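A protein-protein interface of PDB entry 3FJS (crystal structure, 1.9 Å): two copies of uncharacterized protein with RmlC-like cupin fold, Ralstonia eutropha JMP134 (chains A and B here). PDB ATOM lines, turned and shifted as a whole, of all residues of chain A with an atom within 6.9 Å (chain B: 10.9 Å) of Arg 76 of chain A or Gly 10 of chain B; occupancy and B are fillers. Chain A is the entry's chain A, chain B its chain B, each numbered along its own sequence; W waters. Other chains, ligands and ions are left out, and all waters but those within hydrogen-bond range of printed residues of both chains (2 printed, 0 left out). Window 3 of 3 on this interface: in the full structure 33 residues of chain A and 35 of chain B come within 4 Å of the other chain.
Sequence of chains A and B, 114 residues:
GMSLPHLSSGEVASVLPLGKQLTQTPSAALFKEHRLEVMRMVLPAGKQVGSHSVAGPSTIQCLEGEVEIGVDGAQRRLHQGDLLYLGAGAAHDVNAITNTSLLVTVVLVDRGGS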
ATOM      1  N   VAL A  67       4.641   7.522  22.553  1.00  0.00           N
ATOM      2  CA  VAL A  67       3.604   7.072  21.640  1.00  0.00           C
ATOM      3  C   VAL A  67       3.834   5.607  21.332  1.00  0.00           C
ATOM      4  O   VAL A  67       4.972   5.157  21.281  1.00  0.00           O
ATOM      5  CB  VAL A  67       3.659   7.923  20.346  1.00  0.00           C
ATOM      6  CG1 VAL A  67       5.004   7.769  19.601  1.00  0.00           C
ATOM      7  CG2 VAL A  67       2.490   7.617  19.410  1.00  0.00           C
ATOM      8  N   GLU A  68       2.753   4.846  21.215  1.00  0.00           N
ATOM      9  CA  GLU A  68       2.855   3.452  20.837  1.00  0.00           C
ATOM     10  C   GLU A  68       2.360   3.384  19.412  1.00  0.00           C
ATOM     11  O   GLU A  68       1.257   3.847  19.126  1.00  0.00           O
ATOM     12  CB  GLU A  68       2.019   2.554  21.742  1.00  0.00           C
ATOM     13  CG  GLU A  68       2.339   1.095  21.558  1.00  0.00           C
ATOM     14  CD  GLU A  68       1.369   0.205  22.268  1.00  0.00           C
ATOM     15  OE1 GLU A  68       0.169   0.195  21.864  1.00  0.00           O
ATOM     16  OE2 GLU A  68       1.809  -0.515  23.182  1.00  0.00           O
ATOM     17  N   ILE A  69       3.178   2.820  18.528  1.00  0.00           N
ATOM     18  CA  ILE A  69       2.836   2.664  17.117  1.00  0.00           C
ATOM     19  C   ILE A  69       2.768   1.172  16.857  1.00  0.00           C
ATOM     20  O   ILE A  69       3.771   0.464  17.015  1.00  0.00           O
ATOM     21  CB  ILE A  69       3.833   3.355  16.168  1.00  0.00           C
ATOM     22  CG1 ILE A  69       3.837   4.879  16.403  1.00  0.00           C
ATOM     23  CG2 ILE A  69       3.459   3.050  14.674  1.00  0.00           C
ATOM     24  CD1 ILE A  69       5.047   5.514  15.958  1.00  0.00           C
ATOM     25  N   GLY A  70       1.571   0.690  16.514  1.00  0.00           N
ATOM     26  CA  GLY A  70       1.369  -0.715  16.181  1.00  0.00           C
ATOM     27  C   GLY A  70       1.770  -0.926  14.727  1.00  0.00           C
ATOM     28  O   GLY A  70       1.459  -0.083  13.874  1.00  0.00           O
ATOM     29  N   VAL A  71       2.537  -1.988  14.469  1.00  0.00           N
ATOM     30  CA  VAL A  71       2.988  -2.358  13.121  1.00  0.00           C
ATOM     31  C   VAL A  71       2.800  -3.870  12.946  1.00  0.00           C
ATOM     32  O   VAL A  71       2.573  -4.593  13.934  1.00  0.00           O
ATOM     33  CB  VAL A  71       4.472  -2.004  12.887  1.00  0.00           C
ATOM     34  CG1 VAL A  71       4.693  -0.495  12.998  1.00  0.00           C
ATOM     35  CG2 VAL A  71       5.370  -2.781  13.867  1.00  0.00           C
ATOM     36  N   ASP A  72       2.887  -4.350  11.710  1.00  0.00           N
ATOM     37  CA  ASP A  72       2.731  -5.793  11.440  1.00  0.00           C
ATOM     38  C   ASP A  72       3.769  -6.553  12.256  1.00  0.00           C
ATOM     39  O   ASP A  72       4.970  -6.348  12.069  1.00  0.00           O
ATOM     40  CB  ASP A  72       2.911  -6.116   9.953  1.00  0.00           C
ATOM     41  CG  ASP A  72       1.791  -5.565   9.091  1.00  0.00           C
ATOM     42  OD1 ASP A  72       0.602  -5.792   9.414  1.00  0.00           O
ATOM     43  OD2 ASP A  72       2.098  -4.924   8.066  1.00  0.00           O
ATOM     44  N   GLY A  73       3.303  -7.343  13.222  1.00  0.00           N
ATOM     45  CA  GLY A  73       4.176  -8.140  14.066  1.00  0.00           C
ATOM     46  C   GLY A  73       4.760  -7.504  15.316  1.00  0.00           C
ATOM     47  O   GLY A  73       5.521  -8.181  16.033  1.00  0.00           O
ATOM     48  N   ALA A  74       4.427  -6.238  15.604  1.00  0.00           N
ATOM     49  CA  ALA A  74       4.941  -5.568  16.816  1.00  0.00           C
ATOM     50  C   ALA A  74       4.190  -4.290  17.220  1.00  0.00           C
ATOM     51  O   ALA A  74       3.445  -3.717  16.435  1.00  0.00           O
ATOM     52  CB  ALA A  74       6.446  -5.260  16.656  1.00  0.00           C
ATOM     53  N   GLN A  75       4.375  -3.909  18.483  1.00  0.00           N
ATOM     54  CA  GLN A  75       3.838  -2.689  19.071  1.00  0.00           C
ATOM     55  C   GLN A  75       5.082  -1.932  19.520  1.00  0.00           C
ATOM     56  O   GLN A  75       5.710  -2.316  20.507  1.00  0.00           O
ATOM     57  CB  GLN A  75       2.939  -3.014  20.274  1.00  0.00           C
ATOM     58  CG  GLN A  75       1.595  -3.649  19.945  1.00  0.00           C
ATOM     59  CD  GLN A  75       0.595  -2.700  19.264  1.00  0.00           C
ATOM     60  OE1 GLN A  75      -0.209  -3.135  18.430  1.00  0.00           O
ATOM     61  NE2 GLN A  75       0.626  -1.417  19.627  1.00  0.00           N
ATOM     62  N   ARG A  76       5.457  -0.888  18.789  1.00  0.00           N
ATOM     63  CA  ARG A  76       6.664  -0.135  19.095  1.00  0.00           C
ATOM     64  C   ARG A  76       6.354   1.012  20.024  1.00  0.00           C
ATOM     65  O   ARG A  76       5.538   1.840  19.686  1.00  0.00           O
ATOM     66  CB  ARG A  76       7.281   0.443  17.810  1.00  0.00           C
ATOM     67  CG  ARG A  76       7.563  -0.532  16.719  1.00  0.00           C
ATOM     68  CD  ARG A  76       8.450  -1.644  17.199  1.00  0.00           C
ATOM     69  NE  ARG A  76       8.932  -2.465  16.108  1.00  0.00           N
ATOM     70  CZ  ARG A  76       9.642  -3.576  16.272  1.00  0.00           C
ATOM     71  NH1 ARG A  76       9.918  -4.051  17.485  1.00  0.00           N
ATOM     72  NH2 ARG A  76      10.040  -4.246  15.200  1.00  0.00           N
ATOM     73  N   ARG A  77       7.045   1.075  21.159  1.00  0.00           N
ATOM     74  CA  ARG A  77       6.869   2.150  22.114  1.00  0.00           C
ATOM     75  C   ARG A  77       7.993   3.129  21.805  1.00  0.00           C
ATOM     76  O   ARG A  77       9.164   2.803  22.040  1.00  0.00           O
ATOM     77  CB  ARG A  77       6.939   1.628  23.553  1.00  0.00           C
ATOM     78  CG  ARG A  77       6.515   2.640  24.611  1.00  0.00           C
ATOM     79  CD  ARG A  77       5.018   3.034  24.479  1.00  0.00           C
ATOM     80  NE  ARG A  77       4.037   1.986  24.806  1.00  0.00           N
ATOM     81  CZ  ARG A  77       3.498   1.749  26.014  1.00  0.00           C
ATOM     82  NH1 ARG A  77       3.861   2.417  27.114  1.00  0.00           N
ATOM     83  NH2 ARG A  77       2.585   0.798  26.135  1.00  0.00           N
ATOM     84  N   LEU A  78       7.651   4.283  21.242  1.00  0.00           N
ATOM     85  CA  LEU A  78       8.657   5.285  20.903  1.00  0.00           C
ATOM     86  C   LEU A  78       8.778   6.317  22.009  1.00  0.00           C
ATOM     87  O   LEU A  78       7.780   6.758  22.556  1.00  0.00           O
ATOM     88  CB  LEU A  78       8.334   6.021  19.620  1.00  0.00           C
ATOM     89  CG  LEU A  78       7.965   5.289  18.332  1.00  0.00           C
ATOM     90  CD1 LEU A  78       8.083   6.254  17.162  1.00  0.00           C
ATOM     91  CD2 LEU A  78       8.836   4.154  18.123  1.00  0.00           C
ATOM     92  N   LEU A  84      10.939   5.873  13.571  1.00  0.00           N
ATOM     93  CA  LEU A  84      10.348   4.642  13.023  1.00  0.00           C
ATOM     94  C   LEU A  84      10.277   4.749  11.511  1.00  0.00           C
ATOM     95  O   LEU A  84       9.773   5.747  10.985  1.00  0.00           O
ATOM     96  CB  LEU A  84       8.922   4.414  13.568  1.00  0.00           C
ATOM     97  CG  LEU A  84       8.047   3.332  12.937  1.00  0.00           C
ATOM     98  CD1 LEU A  84       8.651   1.990  13.282  1.00  0.00           C
ATOM     99  CD2 LEU A  84       6.614   3.488  13.438  1.00  0.00           C
ATOM    100  N   TYR A  85      10.743   3.705  10.839  1.00  0.00           N
ATOM    101  CA  TYR A  85      10.659   3.578   9.371  1.00  0.00           C
ATOM    102  C   TYR A  85       9.480   2.692   9.038  1.00  0.00           C
ATOM    103  O   TYR A  85       9.353   1.581   9.596  1.00  0.00           O
ATOM    104  CB  TYR A  85      11.949   2.979   8.809  1.00  0.00           C
ATOM    105  CG  TYR A  85      11.848   2.422   7.379  1.00  0.00           C
ATOM    106  CD1 TYR A  85      11.283   3.178   6.351  1.00  0.00           C
ATOM    107  CD2 TYR A  85      12.393   1.184   7.061  1.00  0.00           C
ATOM    108  CE1 TYR A  85      11.185   2.681   5.037  1.00  0.00           C
ATOM    109  CE2 TYR A  85      12.328   0.680   5.734  1.00  0.00           C
ATOM    110  CZ  TYR A  85      11.721   1.430   4.739  1.00  0.00           C
ATOM    111  OH  TYR A  85      11.640   0.954   3.433  1.00  0.00           O
ATOM    112  N   LEU A  86       8.610   3.184   8.153  1.00  0.00           N
ATOM    113  CA  LEU A  86       7.461   2.428   7.641  1.00  0.00           C
ATOM    114  C   LEU A  86       7.587   2.277   6.115  1.00  0.00           C
ATOM    115  O   LEU A  86       7.660   3.264   5.354  1.00  0.00           O
ATOM    116  CB  LEU A  86       6.150   3.116   8.001  1.00  0.00           C
ATOM    117  CG  LEU A  86       5.712   3.070   9.462  1.00  0.00           C
ATOM    118  CD1 LEU A  86       4.636   4.123   9.707  1.00  0.00           C
ATOM    119  CD2 LEU A  86       5.215   1.662   9.824  1.00  0.00           C
ATOM    120  N   GLY A  87       7.577   1.027   5.671  1.00  0.00           N
ATOM    121  CA  GLY A  87       7.665   0.713   4.274  1.00  0.00           C
ATOM    122  C   GLY A  87       6.386   1.155   3.595  1.00  0.00           C
ATOM    123  O   GLY A  87       5.334   1.385   4.266  1.00  0.00           O
ATOM    124  N   ALA A  90       2.794  -0.090   4.559  1.00  0.00           N
ATOM    125  CA  ALA A  90       2.909  -0.742   5.882  1.00  0.00           C
ATOM    126  C   ALA A  90       1.795  -0.260   6.793  1.00  0.00           C
ATOM    127  O   ALA A  90       1.696   0.936   7.088  1.00  0.00           O
ATOM    128  CB  ALA A  90       4.279  -0.481   6.521  1.00  0.00           C
ATOM    129  N   HIS B   6      20.800  -1.674   9.236  1.00  0.00           N
ATOM    130  CA  HIS B   6      19.794  -0.822   8.588  1.00  0.00           C
ATOM    131  C   HIS B   6      18.416  -1.220   9.114  1.00  0.00           C
ATOM    132  O   HIS B   6      18.182  -2.381   9.401  1.00  0.00           O
ATOM    133  CB  HIS B   6      19.840  -1.023   7.056  1.00  0.00           C
ATOM    134  CG  HIS B   6      20.897  -0.212   6.358  1.00  0.00           C
ATOM    135  ND1 HIS B   6      22.035   0.242   6.994  1.00  0.00           N
ATOM    136  CD2 HIS B   6      21.023   0.162   5.061  1.00  0.00           C
ATOM    137  CE1 HIS B   6      22.789   0.897   6.131  1.00  0.00           C
ATOM    138  NE2 HIS B   6      22.197   0.862   4.950  1.00  0.00           N
ATOM    139  N   LEU B   7      17.513  -0.261   9.238  1.00  0.00           N
ATOM    140  CA  LEU B   7      16.140  -0.561   9.639  1.00  0.00           C
ATOM    141  C   LEU B   7      15.342  -1.161   8.470  1.00  0.00           C
ATOM    142  O   LEU B   7      15.547  -0.736   7.317  1.00  0.00           O
ATOM    143  CB  LEU B   7      15.383   0.724   9.990  1.00  0.00           C
ATOM    144  CG  LEU B   7      15.918   1.710  11.001  1.00  0.00           C
ATOM    145  CD1 LEU B   7      14.986   2.923  11.001  1.00  0.00           C
ATOM    146  CD2 LEU B   7      16.049   1.048  12.380  1.00  0.00           C
ATOM    147  N   SER B   8      14.469  -2.128   8.786  1.00  0.00           N
ATOM    148  CA  SER B   8      13.500  -2.676   7.831  1.00  0.00           C
ATOM    149  C   SER B   8      12.173  -2.060   8.290  1.00  0.00           C
ATOM    150  O   SER B   8      12.142  -1.393   9.330  1.00  0.00           O
ATOM    151  CB  SER B   8      13.462  -4.198   7.851  1.00  0.00           C
ATOM    152  OG  SER B   8      13.035  -4.681   9.103  1.00  0.00           O
ATOM    153  N   SER B   9      11.090  -2.271   7.538  1.00  0.00           N
ATOM    154  CA  SER B   9       9.797  -1.652   7.897  1.00  0.00           C
ATOM    155  C   SER B   9       9.359  -2.045   9.315  1.00  0.00           C
ATOM    156  O   SER B   9       9.468  -3.221   9.698  1.00  0.00           O
ATOM    157  CB  SER B   9       8.709  -2.002   6.908  1.00  0.00           C
ATOM    158  OG  SER B   9       7.508  -1.359   7.285  1.00  0.00           O
ATOM    159  N   GLY B  10       8.912  -1.060  10.083  1.00  0.00           N
ATOM    160  CA  GLY B  10       8.489  -1.272  11.473  1.00  0.00           C
ATOM    161  C   GLY B  10       9.587  -1.151  12.521  1.00  0.00           C
ATOM    162  O   GLY B  10       9.287  -1.212  13.713  1.00  0.00           O
ATOM    163  N   GLU B  11      10.835  -0.935  12.097  1.00  0.00           N
ATOM    164  CA  GLU B  11      11.971  -0.839  13.019  1.00  0.00           C
ATOM    165  C   GLU B  11      12.305   0.581  13.397  1.00  0.00           C
ATOM    166  O   GLU B  11      11.945   1.528  12.684  1.00  0.00           O
ATOM    167  CB  GLU B  11      13.177  -1.575  12.477  1.00  0.00           C
ATOM    168  CG  GLU B  11      12.853  -3.080  12.374  1.00  0.00           C
ATOM    169  CD  GLU B  11      13.980  -3.943  11.905  1.00  0.00           C
ATOM    170  OE1 GLU B  11      14.958  -3.415  11.334  1.00  0.00           O
ATOM    171  OE2 GLU B  11      13.831  -5.184  12.059  1.00  0.00           O
ATOM    172  N   VAL B  12      13.009   0.707  14.523  1.00  0.00           N
ATOM    173  CA  VAL B  12      13.269   1.978  15.146  1.00  0.00           C
ATOM    174  C   VAL B  12      14.755   2.232  15.415  1.00  0.00           C
ATOM    175  O   VAL B  12      15.497   1.320  15.844  1.00  0.00           O
ATOM    176  CB  VAL B  12      12.491   2.059  16.487  1.00  0.00           C
ATOM    177  CG1 VAL B  12      12.747   3.395  17.221  1.00  0.00           C
ATOM    178  CG2 VAL B  12      10.982   1.824  16.267  1.00  0.00           C
ATOM    179  N   ALA B  13      15.154   3.483  15.219  1.00  0.00           N
ATOM    180  CA  ALA B  13      16.497   3.988  15.505  1.00  0.00           C
ATOM    181  C   ALA B  13      16.362   5.222  16.393  1.00  0.00           C
ATOM    182  O   ALA B  13      15.379   5.961  16.267  1.00  0.00           O
ATOM    183  CB  ALA B  13      17.192   4.388  14.210  1.00  0.00           C
ATOM    184  N   LEU B  30      20.473   5.228   8.368  1.00  0.00           N
ATOM    185  CA  LEU B  30      19.429   4.541   9.173  1.00  0.00           C
ATOM    186  C   LEU B  30      18.845   3.479   8.274  1.00  0.00           C
ATOM    187  O   LEU B  30      18.654   2.339   8.680  1.00  0.00           O
ATOM    188  CB  LEU B  30      18.289   5.452   9.656  1.00  0.00           C
ATOM    189  CG  LEU B  30      18.455   6.248  10.957  1.00  0.00           C
ATOM    190  CD1 LEU B  30      19.499   7.345  10.840  1.00  0.00           C
ATOM    191  CD2 LEU B  30      17.100   6.843  11.366  1.00  0.00           C
ATOM    192  N   PHE B  31      18.561   3.856   7.030  1.00  0.00           N
ATOM    193  CA  PHE B  31      18.081   2.918   6.001  1.00  0.00           C
ATOM    194  C   PHE B  31      18.155   3.553   4.637  1.00  0.00           C
ATOM    195  O   PHE B  31      18.178   4.797   4.527  1.00  0.00           O
ATOM    196  CB  PHE B  31      16.645   2.448   6.249  1.00  0.00           C
ATOM    197  CG  PHE B  31      15.624   3.530   6.123  1.00  0.00           C
ATOM    198  CD1 PHE B  31      15.012   3.806   4.870  1.00  0.00           C
ATOM    199  CD2 PHE B  31      15.254   4.262   7.248  1.00  0.00           C
ATOM    200  CE1 PHE B  31      14.040   4.862   4.732  1.00  0.00           C
ATOM    201  CE2 PHE B  31      14.299   5.281   7.132  1.00  0.00           C
ATOM    202  CZ  PHE B  31      13.692   5.590   5.864  1.00  0.00           C
ATOM    203  N   GLU B  33      16.269   2.677   0.867  1.00  0.00           N
ATOM    204  CA  GLU B  33      15.352   1.871   0.099  1.00  0.00           C
ATOM    205  C   GLU B  33      15.203   2.584  -1.237  1.00  0.00           C
ATOM    206  O   GLU B  33      15.748   3.672  -1.444  1.00  0.00           O
ATOM    207  CB  GLU B  33      14.030   1.657   0.847  1.00  0.00           C
ATOM    208  CG  GLU B  33      13.204   2.927   1.134  1.00  0.00           C
ATOM    209  CD  GLU B  33      11.781   2.784   0.661  1.00  0.00           C
ATOM    210  OE1 GLU B  33      10.930   2.293   1.449  1.00  0.00           O
ATOM    211  OE2 GLU B  33      11.543   3.095  -0.534  1.00  0.00           O
HETATM  212  O   HOH W   1       9.301  -4.532  12.295  1.00  0.00           O
HETATM  213  O   HOH W   2       6.576  -4.647  10.921  1.00  0.00           O
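No position is printed for both chains.
Among the printed residues, merely in contact across the chains: Leu 78 of chain A with Val 12 of chain B (3.7 Å), Leu 84 of chain A with Gly 10 of chain B (3.3 Å), Leu 84 of chain A with Glu 11 of chain B (3.4 Å), Leu 84 of chain A with Val 12 of chain B (3.8 Å), Tyr 85 of chain A with Leu 7 of chain B (3.7 Å), Tyr 85 of chain A with Ser 8 of chain B (3.4 Å), Tyr 85 of chain A with Ser 9 of chain B (3.6 Å), Tyr 85 of chain A with Phe 31 of chain B (3.4 Å), Leu 86 of chain A with Ser 9 of chain B (3.8 Å) and Ala 90 of chain A with Ser 9 of chain B (3.4 Å).
Water W2 bridges the backbone carbonyl oxygen of Asp 72 of chain A and the backbone carbonyl oxygen of Ser 9 of chain B.
Water W1 bridges the backbone carbonyl oxygen of Ser 9 of chain B (2.9 Å) and the guanidinium group of Arg 76 of chain A (3.0 Å).
The backbone NH (N) of Gly 87 of chain A is in hydrogen-bond range of the side-chain hydroxyl (OG) of Ser 9 of chain B, 2.9 Å away.
The backbone NH (N) of Gly 10 of chain B is in hydrogen-bond range of the backbone carbonyl oxygen (O) of Tyr 85 of chain A.
The backbone carbonyl oxygen (O) of Glu 11 of chain B sits at hydrogen-bond distance from the backbone NH (N) of Tyr 85 of chain A, at 3.1 Å.
NE of Arg 76 of chain A lies within hydrogen-bond range of O of Gly 10 of chain B.
The side-chain hydroxyl of Tyr 85 of chain A sits at hydrogen-bond distance from the side-chain carboxylate of Glu 33 of chain B (2.5 Å).
Hydrophobic or aromatic side chains of chain B within 4 Å of the printed part of chain A: Leu 7, Val 12 and Phe 31.
Of the 17 printed residues of chain A, 7 touch a printed residue of chain B.
Among the printed residues, 15 pairs touch across the chains.
Among the printed residues, no Asp or Glu carboxylate lies within 4 Å of a Lys or Arg side-chain nitrogen of the other chain.
No residue of chain B comes within 4 Å of Ile 69 of chain A.
No residue of chain B comes within 4 Å of Gly 70 of chain A.
No residue of chain B comes within 4 Å of Val 71 of chain A.
No residue of chain B comes within 4 Å of Ala 74 of chain A.
No residue of chain B comes within 4 Å of Gln 75 of chain A.
Printed residues of chain B within 4 Å of Arg 76 of chain A: Gly 10 (2.7 Å).
Arg 77 of chain A touches none of the printed residues of chain B.
Printed residues of chain B within 4 Å of Leu 84 of chain A: Gly 10, Glu 11 and Val 12.
Of the printed residues of chain B, Leu 86 of chain A touches Ser 9.
Printed residues of chain A within 4 Å of Ser 9 of chain B: Tyr 85 (3.6 Å), Leu 86 (3.8 Å), Gly 87 (2.9 Å) and Ala 90 (3.4 Å).
Leu 30 of chain B touches none of the printed residues of chain A.
The nearest printed residue of chain B that does not touch Arg 76 of chain A is Glu 11 of chain B (4.2 Å).
The nearest residue of chain A that does not touch Gly 10 of chain B is Val 71 of chain A (4.2 Å).
The nearest printed residue of chain B that does not touch Ala 90 of chain A is Gly 10 of chain B (5.9 Å).
The backbone NH (N) of Ser 8 of chain B is in hydrogen-bond range of the side-chain carboxylate (OE1) of Glu 11 of chain B (2.9 Å).
O of Leu 30 of chain B is in hydrogen-bond range of N of Leu 7 of chain B, 2.9 Å away.
O of Val 67 of chain A sits at hydrogen-bond distance from N of Leu 78 of chain A, at 2.8 Å.
O of Ile 69 of chain A is in hydrogen-bond range of N of Arg 76 of chain A (2.8 Å).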
